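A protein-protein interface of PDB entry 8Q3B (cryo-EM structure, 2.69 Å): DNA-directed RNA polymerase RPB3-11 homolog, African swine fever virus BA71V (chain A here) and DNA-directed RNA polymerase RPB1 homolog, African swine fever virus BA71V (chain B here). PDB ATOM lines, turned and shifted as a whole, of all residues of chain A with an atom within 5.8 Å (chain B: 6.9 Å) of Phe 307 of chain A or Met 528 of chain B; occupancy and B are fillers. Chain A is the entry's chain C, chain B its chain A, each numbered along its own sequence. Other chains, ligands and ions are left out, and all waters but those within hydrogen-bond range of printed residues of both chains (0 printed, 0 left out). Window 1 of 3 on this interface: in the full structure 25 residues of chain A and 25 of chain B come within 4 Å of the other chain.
O of Ile 305 of chain A sits at hydrogen-bond distance from NZ of Lys 524 of chain B, at 3.0 Å. SG of Cys 540 of chain B is in hydrogen-bond range of OG of Ser 306 of chain A, at 3.0 Å. The backbone carbonyl oxygen of Ser 306 of chain A is in hydrogen-bond range of the backbone NH of Phe 541 of chain B (3.0 Å).
The backbone carbonyl oxygen (O) of Phe 541 of chain B sits at hydrogen-bond distance from the side-chain amino group (NZ) of Lys 524 of chain B, at 3.3 Å. The side-chain sulfur of Cys 540 of chain B lies close to the backbone NH of Ala 542 of chain B (3.7 Å). O of Ile 324 of chain A sits close to N of Ser 306 of chain A. The backbone carbonyl oxygen (O) of Phe 307 of chain A sits at hydrogen-bond distance from the backbone NH (N) of Ile 324 of chain A, 2.9 Å away. The backbone carbonyl oxygen (O) of Gly 309 of chain A is in hydrogen-bond range of the backbone NH (N) of Thr 322 of chain A (2.9 Å).
Lys 524 of chain B touches Tyr 299 of chain A. Tyr 299 of chain A touches Leu 525 of chain B (CD2 to CD1, 3.8 Å). O of Ile 305 of chain A touches O of Phe 541 of chain B (3.8 Å). O of Ser 306 of chain A touches O of Pro 539 of chain B, 3.96 Å away. Ser 306 of chain A touches Ala 542 of chain B. Met 528 of chain B touches Phe 307 of chain A (O to CE1, 3.4 Å). Phe 307 of chain A touches Pro 538 of chain B. Val 308 of chain A touches Met 528 of chain B. Gly 309 of chain A touches Gln 532 of chain B (CA to OE1, 3.9 Å). Ile 324 of chain A touches Pro 538 of chain B (CD1 to CG, 3.9 Å).
Of the printed residues of chain B, Ile 324 of chain A touches Pro 538. Of chain A, only Phe 307 (3.4 Å) and Val 308 (3.3 Å) come within 4 Å of Met 528 of chain B. Printed residues of chain A within 4 Å of Pro 538 of chain B: Phe 307 (3.6 Å) and Ile 324 (3.9 Å). Printed residues of chain A within 4 Å of Cys 540 of chain B: Ser 306. Printed residues of chain A within 4 Å of Phe 541 of chain B: Ile 305 and Ser 306. Printed residues of chain A within 4 Å of Ala 542 of chain B: Ser 306 (3.9 Å). Leu 550 of chain B touches none of the printed residues of chain A. The nearest printed residue of chain B that does not touch Phe 307 of chain A is Phe 541 of chain B (4.1 Å). The nearest residue of chain A that does not touch Met 528 of chain B is Tyr 299 of chain A (4.3 Å). The nearest printed residue of chain A that does not touch Gln 532 of chain B is Phe 307 of chain A (4.3 Å).
Hydrophobic or aromatic side chains of chain B that line the printed part of chain A: Leu 525, Met 528, Pro 538 and Phe 541. Hydrophobic or aromatic side chains of chain A that line the printed part of chain B: Tyr 299, Phe 307, Val 308 and Ile 324. Among the printed residues, 13 pairs touch across the chains. Among the printed residues, no Asp or Glu carboxylate lies within 4 Å of a Lys or Arg side-chain nitrogen of the other chain.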
ATOM      1  N   TYR A 299     -15.103 -14.466   4.679  1.00  0.00           N
ATOM      2  CA  TYR A 299     -15.948 -14.074   3.558  1.00  0.00           C
ATOM      3  C   TYR A 299     -16.507 -15.296   2.842  1.00  0.00           C
ATOM      4  O   TYR A 299     -17.684 -15.318   2.463  1.00  0.00           O
ATOM      5  CB  TYR A 299     -15.147 -13.201   2.596  1.00  0.00           C
ATOM      6  CG  TYR A 299     -15.830 -12.936   1.277  1.00  0.00           C
ATOM      7  CD1 TYR A 299     -16.970 -12.151   1.208  1.00  0.00           C
ATOM      8  CD2 TYR A 299     -15.325 -13.463   0.098  1.00  0.00           C
ATOM      9  CE1 TYR A 299     -17.591 -11.904   0.003  1.00  0.00           C
ATOM     10  CE2 TYR A 299     -15.941 -13.222  -1.111  1.00  0.00           C
ATOM     11  CZ  TYR A 299     -17.072 -12.441  -1.154  1.00  0.00           C
ATOM     12  OH  TYR A 299     -17.686 -12.198  -2.359  1.00  0.00           O
ATOM     13  N   ILE A 305     -22.283 -11.741   4.342  1.00  0.00           N
ATOM     14  CA  ILE A 305     -21.757 -10.983   5.467  1.00  0.00           C
ATOM     15  C   ILE A 305     -21.964  -9.494   5.227  1.00  0.00           C
ATOM     16  O   ILE A 305     -21.768  -8.990   4.113  1.00  0.00           O
ATOM     17  CB  ILE A 305     -20.270 -11.313   5.678  1.00  0.00           C
ATOM     18  CG1 ILE A 305     -19.785 -10.760   7.014  1.00  0.00           C
ATOM     19  CG2 ILE A 305     -19.428 -10.767   4.534  1.00  0.00           C
ATOM     20  CD1 ILE A 305     -18.674 -11.569   7.620  1.00  0.00           C
ATOM     21  N   SER A 306     -22.371  -8.780   6.279  1.00  0.00           N
ATOM     22  CA  SER A 306     -22.558  -7.340   6.155  1.00  0.00           C
ATOM     23  C   SER A 306     -21.245  -6.644   5.825  1.00  0.00           C
ATOM     24  O   SER A 306     -21.206  -5.751   4.973  1.00  0.00           O
ATOM     25  CB  SER A 306     -23.157  -6.772   7.441  1.00  0.00           C
ATOM     26  OG  SER A 306     -23.701  -5.484   7.222  1.00  0.00           O
ATOM     27  N   PHE A 307     -20.158  -7.041   6.485  1.00  0.00           N
ATOM     28  CA  PHE A 307     -18.856  -6.463   6.179  1.00  0.00           C
ATOM     29  C   PHE A 307     -17.776  -7.263   6.887  1.00  0.00           C
ATOM     30  O   PHE A 307     -17.968  -7.698   8.022  1.00  0.00           O
ATOM     31  CB  PHE A 307     -18.790  -4.992   6.612  1.00  0.00           C
ATOM     32  CG  PHE A 307     -17.485  -4.322   6.286  1.00  0.00           C
ATOM     33  CD1 PHE A 307     -17.302  -3.691   5.069  1.00  0.00           C
ATOM     34  CD2 PHE A 307     -16.445  -4.317   7.199  1.00  0.00           C
ATOM     35  CE1 PHE A 307     -16.106  -3.073   4.768  1.00  0.00           C
ATOM     36  CE2 PHE A 307     -15.248  -3.700   6.901  1.00  0.00           C
ATOM     37  CZ  PHE A 307     -15.079  -3.077   5.685  1.00  0.00           C
ATOM     38  N   VAL A 308     -16.651  -7.458   6.209  1.00  0.00           N
ATOM     39  CA  VAL A 308     -15.457  -8.021   6.834  1.00  0.00           C
ATOM     40  C   VAL A 308     -14.243  -7.370   6.195  1.00  0.00           C
ATOM     41  O   VAL A 308     -14.148  -7.276   4.969  1.00  0.00           O
ATOM     42  CB  VAL A 308     -15.398  -9.559   6.710  1.00  0.00           C
ATOM     43  CG1 VAL A 308     -15.371  -9.995   5.256  1.00  0.00           C
ATOM     44  CG2 VAL A 308     -14.189 -10.103   7.455  1.00  0.00           C
ATOM     45  N   GLY A 309     -13.318  -6.907   7.030  1.00  0.00           N
ATOM     46  CA  GLY A 309     -12.130  -6.247   6.522  1.00  0.00           C
ATOM     47  C   GLY A 309     -11.023  -6.295   7.545  1.00  0.00           C
ATOM     48  O   GLY A 309     -11.234  -6.653   8.704  1.00  0.00           O
ATOM     49  N   THR A 322     -12.100  -6.321  11.420  1.00  0.00           N
ATOM     50  CA  THR A 322     -13.455  -5.899  11.751  1.00  0.00           C
ATOM     51  C   THR A 322     -14.452  -6.775  11.010  1.00  0.00           C
ATOM     52  O   THR A 322     -14.332  -6.970   9.794  1.00  0.00           O
ATOM     53  CB  THR A 322     -13.675  -4.430  11.382  1.00  0.00           C
ATOM     54  OG1 THR A 322     -12.664  -3.622  11.998  1.00  0.00           O
ATOM     55  CG2 THR A 322     -15.045  -3.958  11.840  1.00  0.00           C
ATOM     56  N   ILE A 323     -15.431  -7.304  11.744  1.00  0.00           N
ATOM     57  CA  ILE A 323     -16.477  -8.155  11.185  1.00  0.00           C
ATOM     58  C   ILE A 323     -17.820  -7.638  11.680  1.00  0.00           C
ATOM     59  O   ILE A 323     -18.070  -7.614  12.890  1.00  0.00           O
ATOM     60  CB  ILE A 323     -16.299  -9.631  11.584  1.00  0.00           C
ATOM     61  CG1 ILE A 323     -14.897 -10.137  11.237  1.00  0.00           C
ATOM     62  CG2 ILE A 323     -17.327 -10.491  10.884  1.00  0.00           C
ATOM     63  CD1 ILE A 323     -14.297 -11.021  12.303  1.00  0.00           C
ATOM     64  N   ILE A 324     -18.689  -7.246  10.753  1.00  0.00           N
ATOM     65  CA  ILE A 324     -20.056  -6.837  11.054  1.00  0.00           C
ATOM     66  C   ILE A 324     -20.990  -7.821  10.367  1.00  0.00           C
ATOM     67  O   ILE A 324     -20.879  -8.041   9.155  1.00  0.00           O
ATOM     68  CB  ILE A 324     -20.341  -5.400  10.583  1.00  0.00           C
ATOM     69  CG1 ILE A 324     -19.261  -4.445  11.094  1.00  0.00           C
ATOM     70  CG2 ILE A 324     -21.717  -4.952  11.056  1.00  0.00           C
ATOM     71  CD1 ILE A 324     -19.416  -3.023  10.603  1.00  0.00           C
ATOM     72  N   HIS A 325     -21.906  -8.411  11.136  1.00  0.00           N
ATOM     73  CA  HIS A 325     -22.806  -9.411  10.576  1.00  0.00           C
ATOM     74  C   HIS A 325     -24.153  -9.373  11.281  1.00  0.00           C
ATOM     75  O   HIS A 325     -24.219  -9.172  12.494  1.00  0.00           O
ATOM     76  CB  HIS A 325     -22.212 -10.819  10.685  1.00  0.00           C
ATOM     77  CG  HIS A 325     -22.993 -11.859   9.946  1.00  0.00           C
ATOM     78  ND1 HIS A 325     -23.205 -13.126  10.445  1.00  0.00           N
ATOM     79  CD2 HIS A 325     -23.619 -11.819   8.746  1.00  0.00           C
ATOM     80  CE1 HIS A 325     -23.925 -13.822   9.584  1.00  0.00           C
ATOM     81  NE2 HIS A 325     -24.189 -13.052   8.543  1.00  0.00           N
ATOM     82  N   MET B 522     -16.387  -4.235  -9.881  1.00  0.00           N
ATOM     83  CA  MET B 522     -15.661  -5.049  -8.920  1.00  0.00           C
ATOM     84  C   MET B 522     -16.654  -5.933  -8.182  1.00  0.00           C
ATOM     85  O   MET B 522     -17.830  -5.590  -8.050  1.00  0.00           O
ATOM     86  CB  MET B 522     -14.882  -4.192  -7.913  1.00  0.00           C
ATOM     87  CG  MET B 522     -15.697  -3.078  -7.275  1.00  0.00           C
ATOM     88  SD  MET B 522     -14.674  -1.803  -6.518  1.00  0.00           S
ATOM     89  CE  MET B 522     -14.546  -0.633  -7.867  1.00  0.00           C
ATOM     90  N   ASN B 523     -16.171  -7.075  -7.702  1.00  0.00           N
ATOM     91  CA  ASN B 523     -17.022  -7.988  -6.956  1.00  0.00           C
ATOM     92  C   ASN B 523     -17.249  -7.448  -5.544  1.00  0.00           C
ATOM     93  O   ASN B 523     -16.772  -6.372  -5.175  1.00  0.00           O
ATOM     94  CB  ASN B 523     -16.409  -9.386  -6.922  1.00  0.00           C
ATOM     95  CG  ASN B 523     -14.987  -9.390  -6.403  1.00  0.00           C
ATOM     96  OD1 ASN B 523     -14.469  -8.363  -5.969  1.00  0.00           O
ATOM     97  ND2 ASN B 523     -14.347 -10.551  -6.445  1.00  0.00           N
ATOM     98  N   LYS B 524     -17.999  -8.205  -4.743  1.00  0.00           N
ATOM     99  CA  LYS B 524     -18.300  -7.764  -3.386  1.00  0.00           C
ATOM    100  C   LYS B 524     -17.035  -7.663  -2.542  1.00  0.00           C
ATOM    101  O   LYS B 524     -16.879  -6.717  -1.762  1.00  0.00           O
ATOM    102  CB  LYS B 524     -19.300  -8.721  -2.736  1.00  0.00           C
ATOM    103  CG  LYS B 524     -19.651  -8.381  -1.294  1.00  0.00           C
ATOM    104  CD  LYS B 524     -20.494  -9.471  -0.659  1.00  0.00           C
ATOM    105  CE  LYS B 524     -20.828  -9.145   0.785  1.00  0.00           C
ATOM    106  NZ  LYS B 524     -21.843 -10.071   1.352  1.00  0.00           N
ATOM    107  N   LEU B 525     -16.123  -8.626  -2.681  1.00  0.00           N
ATOM    108  CA  LEU B 525     -14.946  -8.660  -1.819  1.00  0.00           C
ATOM    109  C   LEU B 525     -14.091  -7.412  -2.000  1.00  0.00           C
ATOM    110  O   LEU B 525     -13.659  -6.795  -1.021  1.00  0.00           O
ATOM    111  CB  LEU B 525     -14.125  -9.917  -2.105  1.00  0.00           C
ATOM    112  CG  LEU B 525     -12.876 -10.109  -1.242  1.00  0.00           C
ATOM    113  CD1 LEU B 525     -13.247 -10.233   0.228  1.00  0.00           C
ATOM    114  CD2 LEU B 525     -12.089 -11.324  -1.700  1.00  0.00           C
ATOM    115  N   HIS B 526     -13.842  -7.015  -3.249  1.00  0.00           N
ATOM    116  CA  HIS B 526     -12.966  -5.873  -3.490  1.00  0.00           C
ATOM    117  C   HIS B 526     -13.661  -4.559  -3.155  1.00  0.00           C
ATOM    118  O   HIS B 526     -13.028  -3.627  -2.644  1.00  0.00           O
ATOM    119  CB  HIS B 526     -12.487  -5.883  -4.940  1.00  0.00           C
ATOM    120  CG  HIS B 526     -11.465  -6.939  -5.224  1.00  0.00           C
ATOM    121  ND1 HIS B 526     -11.798  -8.262  -5.424  1.00  0.00           N
ATOM    122  CD2 HIS B 526     -10.117  -6.870  -5.332  1.00  0.00           C
ATOM    123  CE1 HIS B 526     -10.699  -8.960  -5.648  1.00  0.00           C
ATOM    124  NE2 HIS B 526      -9.666  -8.140  -5.597  1.00  0.00           N
ATOM    125  N   ALA B 527     -14.963  -4.465  -3.426  1.00  0.00           N
ATOM    126  CA  ALA B 527     -15.710  -3.283  -3.012  1.00  0.00           C
ATOM    127  C   ALA B 527     -15.654  -3.114  -1.501  1.00  0.00           C
ATOM    128  O   ALA B 527     -15.473  -2.001  -0.997  1.00  0.00           O
ATOM    129  CB  ALA B 527     -17.158  -3.385  -3.487  1.00  0.00           C
ATOM    130  N   MET B 528     -15.807  -4.214  -0.764  1.00  0.00           N
ATOM    131  CA  MET B 528     -15.677  -4.171   0.688  1.00  0.00           C
ATOM    132  C   MET B 528     -14.269  -3.764   1.102  1.00  0.00           C
ATOM    133  O   MET B 528     -14.086  -2.918   1.983  1.00  0.00           O
ATOM    134  CB  MET B 528     -16.037  -5.538   1.266  1.00  0.00           C
ATOM    135  CG  MET B 528     -17.443  -5.630   1.823  1.00  0.00           C
ATOM    136  SD  MET B 528     -17.947  -7.307   2.264  1.00  0.00           S
ATOM    137  CE  MET B 528     -16.382  -8.097   2.619  1.00  0.00           C
ATOM    138  N   GLY B 529     -13.255  -4.359   0.469  1.00  0.00           N
ATOM    139  CA  GLY B 529     -11.879  -4.049   0.810  1.00  0.00           C
ATOM    140  C   GLY B 529     -11.495  -2.611   0.542  1.00  0.00           C
ATOM    141  O   GLY B 529     -10.571  -2.095   1.177  1.00  0.00           O
ATOM    142  N   LEU B 530     -12.175  -1.952  -0.397  1.00  0.00           N
ATOM    143  CA  LEU B 530     -11.908  -0.536  -0.627  1.00  0.00           C
ATOM    144  C   LEU B 530     -12.162   0.293   0.626  1.00  0.00           C
ATOM    145  O   LEU B 530     -11.526   1.335   0.818  1.00  0.00           O
ATOM    146  CB  LEU B 530     -12.774  -0.012  -1.775  1.00  0.00           C
ATOM    147  CG  LEU B 530     -12.420  -0.391  -3.214  1.00  0.00           C
ATOM    148  CD1 LEU B 530     -13.195   0.488  -4.178  1.00  0.00           C
ATOM    149  CD2 LEU B 530     -10.930  -0.278  -3.482  1.00  0.00           C
ATOM    150  N   PHE B 531     -13.077  -0.150   1.487  1.00  0.00           N
ATOM    151  CA  PHE B 531     -13.525   0.627   2.635  1.00  0.00           C
ATOM    152  C   PHE B 531     -12.829   0.240   3.934  1.00  0.00           C
ATOM    153  O   PHE B 531     -13.211   0.740   4.996  1.00  0.00           O
ATOM    154  CB  PHE B 531     -15.037   0.472   2.809  1.00  0.00           C
ATOM    155  CG  PHE B 531     -15.846   1.269   1.830  1.00  0.00           C
ATOM    156  CD1 PHE B 531     -16.186   2.581   2.101  1.00  0.00           C
ATOM    157  CD2 PHE B 531     -16.274   0.703   0.644  1.00  0.00           C
ATOM    158  CE1 PHE B 531     -16.931   3.314   1.204  1.00  0.00           C
ATOM    159  CE2 PHE B 531     -17.021   1.432  -0.256  1.00  0.00           C
ATOM    160  CZ  PHE B 531     -17.349   2.739   0.025  1.00  0.00           C
ATOM    161  N   GLN B 532     -11.822  -0.631   3.884  1.00  0.00           N
ATOM    162  CA  GLN B 532     -11.247  -1.168   5.112  1.00  0.00           C
ATOM    163  C   GLN B 532     -10.189  -0.265   5.731  1.00  0.00           C
ATOM    164  O   GLN B 532      -9.762  -0.533   6.860  1.00  0.00           O
ATOM    165  CB  GLN B 532     -10.646  -2.550   4.849  1.00  0.00           C
ATOM    166  CG  GLN B 532      -9.375  -2.536   4.027  1.00  0.00           C
ATOM    167  CD  GLN B 532      -9.011  -3.909   3.506  1.00  0.00           C
ATOM    168  OE1 GLN B 532      -9.730  -4.881   3.731  1.00  0.00           O
ATOM    169  NE2 GLN B 532      -7.889  -3.997   2.803  1.00  0.00           N
ATOM    170  N   THR B 533      -9.757   0.789   5.038  1.00  0.00           N
ATOM    171  CA  THR B 533      -8.767   1.717   5.574  1.00  0.00           C
ATOM    172  C   THR B 533      -9.288   3.146   5.657  1.00  0.00           C
ATOM    173  O   THR B 533      -8.496   4.069   5.881  1.00  0.00           O
ATOM    174  CB  THR B 533      -7.489   1.685   4.728  1.00  0.00           C
ATOM    175  OG1 THR B 533      -7.822   1.851   3.345  1.00  0.00           O
ATOM    176  CG2 THR B 533      -6.755   0.368   4.917  1.00  0.00           C
ATOM    177  N   PRO B 538     -18.015   1.216   8.334  1.00  0.00           N
ATOM    178  CA  PRO B 538     -18.184   0.523   7.053  1.00  0.00           C
ATOM    179  C   PRO B 538     -19.642   0.502   6.633  1.00  0.00           C
ATOM    180  O   PRO B 538     -20.536   0.360   7.481  1.00  0.00           O
ATOM    181  CB  PRO B 538     -17.665  -0.895   7.341  1.00  0.00           C
ATOM    182  CG  PRO B 538     -16.893  -0.791   8.605  1.00  0.00           C
ATOM    183  CD  PRO B 538     -17.516   0.310   9.382  1.00  0.00           C
ATOM    184  N   PRO B 539     -19.928   0.638   5.335  1.00  0.00           N
ATOM    185  CA  PRO B 539     -21.320   0.516   4.883  1.00  0.00           C
ATOM    186  C   PRO B 539     -21.797  -0.926   4.929  1.00  0.00           C
ATOM    187  O   PRO B 539     -21.047  -1.816   5.338  1.00  0.00           O
ATOM    188  CB  PRO B 539     -21.280   1.062   3.451  1.00  0.00           C
ATOM    189  CG  PRO B 539     -19.877   0.911   3.013  1.00  0.00           C
ATOM    190  CD  PRO B 539     -19.011   0.974   4.233  1.00  0.00           C
ATOM    191  N   CYS B 540     -23.037  -1.171   4.517  1.00  0.00           N
ATOM    192  CA  CYS B 540     -23.633  -2.499   4.579  1.00  0.00           C
ATOM    193  C   CYS B 540     -23.594  -3.134   3.195  1.00  0.00           C
ATOM    194  O   CYS B 540     -24.099  -2.556   2.226  1.00  0.00           O
ATOM    195  CB  CYS B 540     -25.070  -2.426   5.093  1.00  0.00           C
ATOM    196  SG  CYS B 540     -25.755  -4.022   5.590  1.00  0.00           S
ATOM    197  N   PHE B 541     -22.994  -4.321   3.108  1.00  0.00           N
ATOM    198  CA  PHE B 541     -22.968  -5.109   1.883  1.00  0.00           C
ATOM    199  C   PHE B 541     -23.796  -6.384   2.011  1.00  0.00           C
ATOM    200  O   PHE B 541     -23.616  -7.318   1.225  1.00  0.00           O
ATOM    201  CB  PHE B 541     -21.528  -5.456   1.504  1.00  0.00           C
ATOM    202  CG  PHE B 541     -20.707  -4.269   1.094  1.00  0.00           C
ATOM    203  CD1 PHE B 541     -20.055  -3.501   2.041  1.00  0.00           C
ATOM    204  CD2 PHE B 541     -20.585  -3.923  -0.239  1.00  0.00           C
ATOM    205  CE1 PHE B 541     -19.298  -2.413   1.665  1.00  0.00           C
ATOM    206  CE2 PHE B 541     -19.830  -2.834  -0.618  1.00  0.00           C
ATOM    207  CZ  PHE B 541     -19.187  -2.077   0.335  1.00  0.00           C
ATOM    208  N   ALA B 542     -24.700  -6.440   2.992  1.00  0.00           N
ATOM    209  CA  ALA B 542     -25.488  -7.645   3.214  1.00  0.00           C
ATOM    210  C   ALA B 542     -26.419  -7.955   2.051  1.00  0.00           C
ATOM    211  O   ALA B 542     -26.878  -9.096   1.930  1.00  0.00           O
ATOM    212  CB  ALA B 542     -26.301  -7.507   4.500  1.00  0.00           C
ATOM    213  N   LEU B 550     -20.112  -4.452  -8.644  1.00  0.00           N
ATOM    214  CA  LEU B 550     -20.328  -3.081  -8.203  1.00  0.00           C
ATOM    215  C   LEU B 550     -19.427  -2.145  -8.994  1.00  0.00           C
ATOM    216  O   LEU B 550     -18.250  -2.442  -9.214  1.00  0.00           O
ATOM    217  CB  LEU B 550     -20.036  -2.930  -6.708  1.00  0.00           C
ATOM    218  CG  LEU B 550     -21.051  -3.547  -5.748  1.00  0.00           C
ATOM    219  CD1 LEU B 550     -20.715  -5.001  -5.472  1.00  0.00           C
ATOM    220  CD2 LEU B 550     -21.098  -2.757  -4.454  1.00  0.00           C
ATOM    221  N   VAL B 555     -19.546   2.697  -4.986  1.00  0.00           N
ATOM    222  CA  VAL B 555     -18.807   2.854  -3.736  1.00  0.00           C
ATOM    223  C   VAL B 555     -18.612   4.333  -3.417  1.00  0.00           C
ATOM    224  O   VAL B 555     -18.757   4.761  -2.260  1.00  0.00           O
ATOM    225  CB  VAL B 555     -17.469   2.092  -3.803  1.00  0.00           C
ATOM    226  CG1 VAL B 555     -17.718   0.620  -4.090  1.00  0.00           C
ATOM    227  CG2 VAL B 555     -16.552   2.675  -4.860  1.00  0.00           C
ATOM    228  N   ASN B 642      -6.896   2.683  -2.408  1.00  0.00           N
ATOM    229  CA  ASN B 642      -7.219   1.263  -2.368  1.00  0.00           C
ATOM    230  C   ASN B 642      -7.649   0.749  -3.734  1.00  0.00           C
ATOM    231  O   ASN B 642      -7.367  -0.405  -4.073  1.00  0.00           O
ATOM    232  CB  ASN B 642      -8.315   1.003  -1.336  1.00  0.00           C
ATOM    233  CG  ASN B 642      -7.795   1.041   0.086  1.00  0.00           C
ATOM    234  OD1 ASN B 642      -6.592   1.142   0.316  1.00  0.00           O
ATOM    235  ND2 ASN B 642      -8.703   0.958   1.048  1.00  0.00           N
